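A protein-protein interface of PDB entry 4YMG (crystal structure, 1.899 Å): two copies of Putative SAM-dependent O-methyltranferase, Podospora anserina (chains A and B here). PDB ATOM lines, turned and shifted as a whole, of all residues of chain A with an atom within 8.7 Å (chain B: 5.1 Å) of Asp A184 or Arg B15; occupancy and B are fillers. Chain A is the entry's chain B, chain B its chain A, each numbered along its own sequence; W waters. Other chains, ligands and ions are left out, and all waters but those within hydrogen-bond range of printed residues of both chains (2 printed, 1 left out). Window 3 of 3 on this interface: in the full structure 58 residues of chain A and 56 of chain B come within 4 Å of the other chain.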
ATOM      1  N   LEU A   2     -12.124   3.744   8.236  1.00  0.00           N
ATOM      2  CA  LEU A   2     -11.730   4.923   7.468  1.00  0.00           C
ATOM      3  C   LEU A   2     -12.461   4.975   6.126  1.00  0.00           C
ATOM      4  O   LEU A   2     -12.713   3.944   5.502  1.00  0.00           O
ATOM      5  CB  LEU A   2     -10.217   4.938   7.251  1.00  0.00           C
ATOM      6  CG  LEU A   2      -9.507   6.290   7.386  1.00  0.00           C
ATOM      7  CD1 LEU A   2     -10.142   7.142   8.479  1.00  0.00           C
ATOM      8  CD2 LEU A   2      -8.034   6.052   7.665  1.00  0.00           C
ATOM      9  N   GLY A   3     -12.789   6.188   5.688  1.00  0.00           N
ATOM     10  CA  GLY A   3     -13.725   6.384   4.596  1.00  0.00           C
ATOM     11  C   GLY A   3     -13.141   6.588   3.213  1.00  0.00           C
ATOM     12  O   GLY A   3     -11.938   6.455   3.000  1.00  0.00           O
ATOM     13  N   SER A   4     -14.020   6.912   2.269  1.00  0.00           N
ATOM     14  CA  SER A   4     -13.658   7.033   0.869  1.00  0.00           C
ATOM     15  C   SER A   4     -13.624   8.475   0.387  1.00  0.00           C
ATOM     16  O   SER A   4     -13.484   8.710  -0.808  1.00  0.00           O
ATOM     17  CB  SER A   4     -14.645   6.250  -0.001  1.00  0.00           C
ATOM     18  OG  SER A   4     -14.854   4.947   0.502  1.00  0.00           O
ATOM     19  N   ILE A   5     -13.782   9.432   1.302  1.00  0.00           N
ATOM     20  CA  ILE A   5     -13.927  10.832   0.911  1.00  0.00           C
ATOM     21  C   ILE A   5     -12.774  11.658   1.470  1.00  0.00           C
ATOM     22  O   ILE A   5     -12.478  11.584   2.656  1.00  0.00           O
ATOM     23  CB  ILE A   5     -15.283  11.413   1.401  1.00  0.00           C
ATOM     24  CG1 ILE A   5     -16.450  10.625   0.797  1.00  0.00           C
ATOM     25  CG2 ILE A   5     -15.410  12.886   1.042  1.00  0.00           C
ATOM     26  CD1 ILE A   5     -17.802  10.997   1.394  1.00  0.00           C
ATOM     27  N   PHE A 175     -26.955  14.650  -1.375  1.00  0.00           N
ATOM     28  CA  PHE A 175     -26.371  15.017  -0.078  1.00  0.00           C
ATOM     29  C   PHE A 175     -26.995  16.263   0.567  1.00  0.00           C
ATOM     30  O   PHE A 175     -26.812  16.490   1.758  1.00  0.00           O
ATOM     31  CB  PHE A 175     -24.868  15.274  -0.223  1.00  0.00           C
ATOM     32  CG  PHE A 175     -24.035  14.035  -0.404  1.00  0.00           C
ATOM     33  CD1 PHE A 175     -24.563  12.771  -0.202  1.00  0.00           C
ATOM     34  CD2 PHE A 175     -22.686  14.148  -0.741  1.00  0.00           C
ATOM     35  CE1 PHE A 175     -23.772  11.641  -0.359  1.00  0.00           C
ATOM     36  CE2 PHE A 175     -21.892  13.024  -0.897  1.00  0.00           C
ATOM     37  CZ  PHE A 175     -22.445  11.762  -0.705  1.00  0.00           C
ATOM     38  N   ARG A 177     -25.985  19.294   0.369  1.00  0.00           N
ATOM     39  CA  ARG A 177     -24.827  20.047   0.845  1.00  0.00           C
ATOM     40  C   ARG A 177     -24.199  19.410   2.078  1.00  0.00           C
ATOM     41  O   ARG A 177     -23.328  20.003   2.705  1.00  0.00           O
ATOM     42  CB  ARG A 177     -25.195  21.511   1.136  1.00  0.00           C
ATOM     43  CG  ARG A 177     -25.780  22.261  -0.050  1.00  0.00           C
ATOM     44  CD  ARG A 177     -24.783  22.427  -1.175  1.00  0.00           C
ATOM     45  NE  ARG A 177     -25.205  23.465  -2.117  1.00  0.00           N
ATOM     46  CZ  ARG A 177     -25.654  23.246  -3.349  1.00  0.00           C
ATOM     47  NH1 ARG A 177     -25.736  22.008  -3.827  1.00  0.00           N
ATOM     48  NH2 ARG A 177     -26.012  24.275  -4.115  1.00  0.00           N
ATOM     49  N   GLY A 178     -24.624  18.192   2.402  1.00  0.00           N
ATOM     50  CA  GLY A 178     -24.202  17.528   3.618  1.00  0.00           C
ATOM     51  C   GLY A 178     -25.352  17.235   4.571  1.00  0.00           C
ATOM     52  O   GLY A 178     -25.286  16.298   5.369  1.00  0.00           O
ATOM     53  N   LEU A 179     -26.423  18.013   4.465  1.00  0.00           N
ATOM     54  CA  LEU A 179     -27.485  17.955   5.451  1.00  0.00           C
ATOM     55  C   LEU A 179     -28.349  16.699   5.352  1.00  0.00           C
ATOM     56  O   LEU A 179     -29.098  16.401   6.273  1.00  0.00           O
ATOM     57  CB  LEU A 179     -28.357  19.210   5.358  1.00  0.00           C
ATOM     58  CG  LEU A 179     -27.599  20.484   5.767  1.00  0.00           C
ATOM     59  CD1 LEU A 179     -28.523  21.714   5.854  1.00  0.00           C
ATOM     60  CD2 LEU A 179     -26.848  20.260   7.089  1.00  0.00           C
ATOM     61  N   THR A 180     -28.243  15.954   4.256  1.00  0.00           N
ATOM     62  CA  THR A 180     -28.956  14.678   4.163  1.00  0.00           C
ATOM     63  C   THR A 180     -28.440  13.703   5.223  1.00  0.00           C
ATOM     64  O   THR A 180     -29.205  12.916   5.812  1.00  0.00           O
ATOM     65  CB  THR A 180     -28.799  14.041   2.767  1.00  0.00           C
ATOM     66  OG1 THR A 180     -29.367  14.916   1.791  1.00  0.00           O
ATOM     67  CG2 THR A 180     -29.519  12.661   2.701  1.00  0.00           C
ATOM     68  N   ILE A 181     -27.131  13.776   5.458  1.00  0.00           N
ATOM     69  CA  ILE A 181     -26.439  12.878   6.374  1.00  0.00           C
ATOM     70  C   ILE A 181     -26.670  13.285   7.829  1.00  0.00           C
ATOM     71  O   ILE A 181     -26.930  12.445   8.679  1.00  0.00           O
ATOM     72  CB  ILE A 181     -24.915  12.843   6.097  1.00  0.00           C
ATOM     73  CG1 ILE A 181     -24.612  12.295   4.689  1.00  0.00           C
ATOM     74  CG2 ILE A 181     -24.200  12.007   7.144  1.00  0.00           C
ATOM     75  CD1 ILE A 181     -24.435  13.386   3.615  1.00  0.00           C
ATOM     76  N   GLY A 182     -26.585  14.581   8.116  1.00  0.00           N
ATOM     77  CA  GLY A 182     -26.843  15.051   9.464  1.00  0.00           C
ATOM     78  C   GLY A 182     -26.763  16.564   9.555  1.00  0.00           C
ATOM     79  O   GLY A 182     -26.143  17.203   8.711  1.00  0.00           O
ATOM     80  N   PRO A 183     -27.371  17.139  10.601  1.00  0.00           N
ATOM     81  CA  PRO A 183     -27.511  18.592  10.744  1.00  0.00           C
ATOM     82  C   PRO A 183     -26.170  19.283  10.960  1.00  0.00           C
ATOM     83  O   PRO A 183     -26.074  20.488  10.725  1.00  0.00           O
ATOM     84  CB  PRO A 183     -28.402  18.746  11.990  1.00  0.00           C
ATOM     85  CG  PRO A 183     -28.956  17.382  12.268  1.00  0.00           C
ATOM     86  CD  PRO A 183     -27.940  16.417  11.752  1.00  0.00           C
ATOM     87  N   ASP A 184     -25.163  18.528  11.398  1.00  0.00           N
ATOM     88  CA  ASP A 184     -23.842  19.090  11.677  1.00  0.00           C
ATOM     89  C   ASP A 184     -22.834  18.812  10.555  1.00  0.00           C
ATOM     90  O   ASP A 184     -21.633  19.015  10.735  1.00  0.00           O
ATOM     91  CB  ASP A 184     -23.291  18.547  13.008  1.00  0.00           C
ATOM     92  CG  ASP A 184     -23.086  17.031  12.991  1.00  0.00           C
ATOM     93  OD1 ASP A 184     -23.807  16.326  12.248  1.00  0.00           O
ATOM     94  OD2 ASP A 184     -22.202  16.548  13.731  1.00  0.00           O
ATOM     95  N   CYS A 185     -23.321  18.379   9.395  1.00  0.00           N
ATOM     96  CA  CYS A 185     -22.425  17.951   8.323  1.00  0.00           C
ATOM     97  C   CYS A 185     -22.157  19.025   7.275  1.00  0.00           C
ATOM     98  O   CYS A 185     -21.492  18.752   6.279  1.00  0.00           O
ATOM     99  CB  CYS A 185     -22.986  16.700   7.641  1.00  0.00           C
ATOM    100  SG  CYS A 185     -22.925  15.213   8.696  1.00  0.00           S
ATOM    101  N   ALA A 186     -22.667  20.239   7.490  1.00  0.00           N
ATOM    102  CA  ALA A 186     -22.343  21.353   6.592  1.00  0.00           C
ATOM    103  C   ALA A 186     -22.129  22.671   7.351  1.00  0.00           C
ATOM    104  O   ALA A 186     -22.875  23.637   7.154  1.00  0.00           O
ATOM    105  CB  ALA A 186     -23.439  21.526   5.555  1.00  0.00           C
ATOM    106  N   PRO A 187     -21.112  22.714   8.222  1.00  0.00           N
ATOM    107  CA  PRO A 187     -20.895  23.904   9.064  1.00  0.00           C
ATOM    108  C   PRO A 187     -20.547  25.157   8.255  1.00  0.00           C
ATOM    109  O   PRO A 187     -20.705  26.271   8.749  1.00  0.00           O
ATOM    110  CB  PRO A 187     -19.725  23.488   9.962  1.00  0.00           C
ATOM    111  CG  PRO A 187     -19.041  22.370   9.206  1.00  0.00           C
ATOM    112  CD  PRO A 187     -20.129  21.650   8.495  1.00  0.00           C
ATOM    113  N   TRP A 188     -20.091  24.958   7.024  1.00  0.00           N
ATOM    114  CA  TRP A 188     -19.674  26.046   6.137  1.00  0.00           C
ATOM    115  C   TRP A 188     -20.843  26.690   5.410  1.00  0.00           C
ATOM    116  O   TRP A 188     -20.712  27.780   4.847  1.00  0.00           O
ATOM    117  CB  TRP A 188     -18.696  25.506   5.094  1.00  0.00           C
ATOM    118  CG  TRP A 188     -19.316  24.395   4.298  1.00  0.00           C
ATOM    119  CD1 TRP A 188     -19.338  23.068   4.627  1.00  0.00           C
ATOM    120  CD2 TRP A 188     -20.034  24.512   3.056  1.00  0.00           C
ATOM    121  NE1 TRP A 188     -20.009  22.354   3.669  1.00  0.00           N
ATOM    122  CE2 TRP A 188     -20.448  23.214   2.693  1.00  0.00           C
ATOM    123  CE3 TRP A 188     -20.366  25.586   2.218  1.00  0.00           C
ATOM    124  CZ2 TRP A 188     -21.176  22.959   1.528  1.00  0.00           C
ATOM    125  CZ3 TRP A 188     -21.088  25.331   1.058  1.00  0.00           C
ATOM    126  CH2 TRP A 188     -21.485  24.028   0.724  1.00  0.00           C
ATOM    127  N   ARG A 194     -29.628  27.430   4.607  1.00  0.00           N
ATOM    128  CA  ARG A 194     -29.595  26.246   5.462  1.00  0.00           C
ATOM    129  C   ARG A 194     -30.994  25.627   5.687  1.00  0.00           C
ATOM    130  O   ARG A 194     -31.150  24.413   5.532  1.00  0.00           O
ATOM    131  CB  ARG A 194     -28.921  26.588   6.797  1.00  0.00           C
ATOM    132  CG  ARG A 194     -28.804  25.421   7.793  1.00  0.00           C
ATOM    133  CD  ARG A 194     -28.021  25.857   9.050  1.00  0.00           C
ATOM    134  NE  ARG A 194     -26.626  26.226   8.758  1.00  0.00           N
ATOM    135  CZ  ARG A 194     -25.625  25.355   8.581  1.00  0.00           C
ATOM    136  NH1 ARG A 194     -25.844  24.043   8.641  1.00  0.00           N
ATOM    137  NH2 ARG A 194     -24.391  25.792   8.319  1.00  0.00           N
ATOM    138  N   ASN A 198     -31.739  21.925   4.639  1.00  0.00           N
ATOM    139  CA  ASN A 198     -32.140  21.021   5.720  1.00  0.00           C
ATOM    140  C   ASN A 198     -33.435  20.255   5.376  1.00  0.00           C
ATOM    141  O   ASN A 198     -33.512  19.035   5.540  1.00  0.00           O
ATOM    142  CB  ASN A 198     -32.315  21.797   7.022  1.00  0.00           C
ATOM    143  CG  ASN A 198     -32.669  20.896   8.186  1.00  0.00           C
ATOM    144  OD1 ASN A 198     -31.856  20.068   8.603  1.00  0.00           O
ATOM    145  ND2 ASN A 198     -33.882  21.047   8.715  1.00  0.00           N
ATOM    146  N   GLU B  11     -13.510  13.963  10.252  1.00  0.00           N
ATOM    147  CA  GLU B  11     -14.557  13.190  10.921  1.00  0.00           C
ATOM    148  C   GLU B  11     -15.835  13.156  10.087  1.00  0.00           C
ATOM    149  O   GLU B  11     -16.460  12.112   9.928  1.00  0.00           O
ATOM    150  CB  GLU B  11     -14.846  13.781  12.302  1.00  0.00           C
ATOM    151  CG  GLU B  11     -15.798  12.970  13.151  1.00  0.00           C
ATOM    152  CD  GLU B  11     -17.254  13.409  13.037  1.00  0.00           C
ATOM    153  OE1 GLU B  11     -17.559  14.359  12.278  1.00  0.00           O
ATOM    154  OE2 GLU B  11     -18.094  12.808  13.740  1.00  0.00           O
ATOM    155  N   THR B  12     -16.219  14.306   9.553  1.00  0.00           N
ATOM    156  CA  THR B  12     -17.463  14.409   8.792  1.00  0.00           C
ATOM    157  C   THR B  12     -17.371  13.640   7.471  1.00  0.00           C
ATOM    158  O   THR B  12     -18.324  12.952   7.082  1.00  0.00           O
ATOM    159  CB  THR B  12     -17.825  15.883   8.542  1.00  0.00           C
ATOM    160  OG1 THR B  12     -17.920  16.554   9.811  1.00  0.00           O
ATOM    161  CG2 THR B  12     -19.157  16.004   7.805  1.00  0.00           C
ATOM    162  N   ALA B  13     -16.221  13.724   6.804  1.00  0.00           N
ATOM    163  CA  ALA B  13     -16.007  12.987   5.551  1.00  0.00           C
ATOM    164  C   ALA B  13     -16.218  11.489   5.762  1.00  0.00           C
ATOM    165  O   ALA B  13     -16.869  10.811   4.949  1.00  0.00           O
ATOM    166  CB  ALA B  13     -14.602  13.245   4.997  1.00  0.00           C
ATOM    167  N   ASP B  14     -15.662  10.978   6.856  1.00  0.00           N
ATOM    168  CA  ASP B  14     -15.820   9.568   7.201  1.00  0.00           C
ATOM    169  C   ASP B  14     -17.288   9.240   7.458  1.00  0.00           C
ATOM    170  O   ASP B  14     -17.770   8.180   7.076  1.00  0.00           O
ATOM    171  CB  ASP B  14     -14.974   9.197   8.430  1.00  0.00           C
ATOM    172  CG  ASP B  14     -13.493   9.038   8.104  1.00  0.00           C
ATOM    173  OD1 ASP B  14     -13.124   9.048   6.911  1.00  0.00           O
ATOM    174  OD2 ASP B  14     -12.694   8.901   9.053  1.00  0.00           O
ATOM    175  N   ARG B  15     -18.007  10.155   8.097  1.00  0.00           N
ATOM    176  CA  ARG B  15     -19.419   9.913   8.357  1.00  0.00           C
ATOM    177  C   ARG B  15     -20.245   9.893   7.087  1.00  0.00           C
ATOM    178  O   ARG B  15     -21.164   9.091   6.958  1.00  0.00           O
ATOM    179  CB  ARG B  15     -19.973  10.961   9.316  1.00  0.00           C
ATOM    180  CG  ARG B  15     -19.789  10.543  10.760  1.00  0.00           C
ATOM    181  CD  ARG B  15     -19.986  11.714  11.681  1.00  0.00           C
ATOM    182  NE  ARG B  15     -21.364  12.178  11.687  1.00  0.00           N
ATOM    183  CZ  ARG B  15     -21.704  13.450  11.854  1.00  0.00           C
ATOM    184  NH1 ARG B  15     -20.756  14.365  12.009  1.00  0.00           N
ATOM    185  NH2 ARG B  15     -22.981  13.807  11.846  1.00  0.00           N
ATOM    186  N   VAL B  16     -19.925  10.783   6.156  1.00  0.00           N
ATOM    187  CA  VAL B  16     -20.611  10.806   4.871  1.00  0.00           C
ATOM    188  C   VAL B  16     -20.231   9.553   4.059  1.00  0.00           C
ATOM    189  O   VAL B  16     -21.064   8.998   3.349  1.00  0.00           O
ATOM    190  CB  VAL B  16     -20.294  12.116   4.094  1.00  0.00           C
ATOM    191  CG1 VAL B  16     -20.900  12.097   2.698  1.00  0.00           C
ATOM    192  CG2 VAL B  16     -20.821  13.317   4.875  1.00  0.00           C
ATOM    193  N   SER B  17     -18.987   9.093   4.185  1.00  0.00           N
ATOM    194  CA  SER B  17     -18.587   7.833   3.567  1.00  0.00           C
ATOM    195  C   SER B  17     -19.450   6.694   4.086  1.00  0.00           C
ATOM    196  O   SER B  17     -19.954   5.882   3.312  1.00  0.00           O
ATOM    197  CB  SER B  17     -17.114   7.500   3.853  1.00  0.00           C
ATOM    198  OG  SER B  17     -16.243   8.273   3.060  1.00  0.00           O
ATOM    199  N   ALA B  18     -19.589   6.628   5.408  1.00  0.00           N
ATOM    200  CA  ALA B  18     -20.389   5.580   6.032  1.00  0.00           C
ATOM    201  C   ALA B  18     -21.854   5.662   5.568  1.00  0.00           C
ATOM    202  O   ALA B  18     -22.515   4.633   5.382  1.00  0.00           O
ATOM    203  CB  ALA B  18     -20.293   5.666   7.567  1.00  0.00           C
ATOM    204  N   TYR B  19     -22.357   6.878   5.384  1.00  0.00           N
ATOM    205  CA  TYR B  19     -23.721   7.071   4.882  1.00  0.00           C
ATOM    206  C   TYR B  19     -23.866   6.480   3.481  1.00  0.00           C
ATOM    207  O   TYR B  19     -24.844   5.788   3.180  1.00  0.00           O
ATOM    208  CB  TYR B  19     -24.096   8.562   4.868  1.00  0.00           C
ATOM    209  CG  TYR B  19     -25.547   8.798   4.497  1.00  0.00           C
ATOM    210  CD1 TYR B  19     -26.549   8.768   5.470  1.00  0.00           C
ATOM    211  CD2 TYR B  19     -25.920   9.013   3.171  1.00  0.00           C
ATOM    212  CE1 TYR B  19     -27.883   8.971   5.134  1.00  0.00           C
ATOM    213  CE2 TYR B  19     -27.248   9.214   2.823  1.00  0.00           C
ATOM    214  CZ  TYR B  19     -28.223   9.179   3.809  1.00  0.00           C
ATOM    215  OH  TYR B  19     -29.528   9.389   3.461  1.00  0.00           O
HETATM  216  O   HOH W   1     -25.452  11.642  11.174  1.00  0.00           O
HETATM  217  O   HOH W   2     -18.997  18.912  10.128  1.00  0.00           O
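Leu A2 touches Asp B14 (CD1 to OD2, 3.2 Å). CA of Gly A3 touches OG of Ser B17 (3.5 Å). Ile A5 touches Ala B13. Ile A5 touches Val B16. Phe A175 touches Val B16. Thr A180 touches Tyr B19 (CG2 to OH, 3.4 Å). CG2 of Val B16 touches CD1 of Ile A181, at 3.8 Å. CG of Tyr B19 touches CG1 of Ile A181, at 3.6 Å. CG2 of Thr B12 touches CA of Cys A185, 3.8 Å away.
OD1 of Asp B14 sits at hydrogen-bond distance from N of Gly A3, 3.1 Å away. NH2 of Arg B15 is in salt-bridge range of OD1 of Asp A184 (2.7 Å). The side-chain sulfur (SG) of Cys A185 is in hydrogen-bond range of the guanidinium group (NH2) of Arg B15 (3.4 Å). The backbone NH (N) of Ser A4 is in hydrogen-bond range of the side-chain hydroxyl (OG) of Ser B17, 2.7 Å away. The side-chain hydroxyl of Ser B17 sits at hydrogen-bond distance from the backbone NH of Ile A5 (3.2 Å).
Among the printed residues, 14 pairs touch across the chains. Among the printed residues, Asp or Glu carboxylates within 4 Å of a Lys or Arg side-chain nitrogen of the other chain: Asp A184 with Arg B15 (2.7 Å).
Printed residues of chain B within 4 Å of Leu A2: Asp B14 (3.2 Å). Of the printed residues of chain B, Thr A180 touches Tyr B19. Pro A183 touches none of the printed residues of chain B. Of chain B, only Arg B15 comes within 4 Å of Asp A184. Trp A188 touches none of the printed residues of chain B. Of chain A, only Asp A184 and Cys A185 come within 4 Å of Arg B15. Of the printed residues of chain A, Tyr B19 touches Thr A180 (3.4 Å) and Ile A181 (3.6 Å). The nearest residue of chain A that does not touch Arg B15 is Ile A181 (4.2 Å). The nearest printed residue of chain A that does not touch Asp B14 is Ile A5 (5.0 Å).
The side-chain hydroxyl (OG1) of Thr B12 sits at hydrogen-bond distance from the side-chain carboxylate (OE1) of Glu B11 (3.3 Å). OE1 of Glu B11 lies within salt-bridge range of NH1 of Arg B15 (3.2 Å). O of Ala B13 is in hydrogen-bond range of OG of Ser B17, 3.2 Å away. N of Thr A180 is in hydrogen-bond range of O of Phe A175 (2.9 Å). The side-chain sulfur of Cys A185 lies within hydrogen-bond range of the backbone NH of Gly A182 (3.8 Å).
No position is printed for both chains. Of the 14 pairs that touch across the chains among the printed residues, none has its exchanged pair printed and touching as well.
Water W2 bridges the side-chain hydroxyl of Thr B12 (2.6 Å) and the backbone carbonyl oxygen of Asp A184 (2.7 Å). Water W1 bridges O of Ile A181 (3.0 Å) and NH2 of Arg B15 (3.4 Å).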
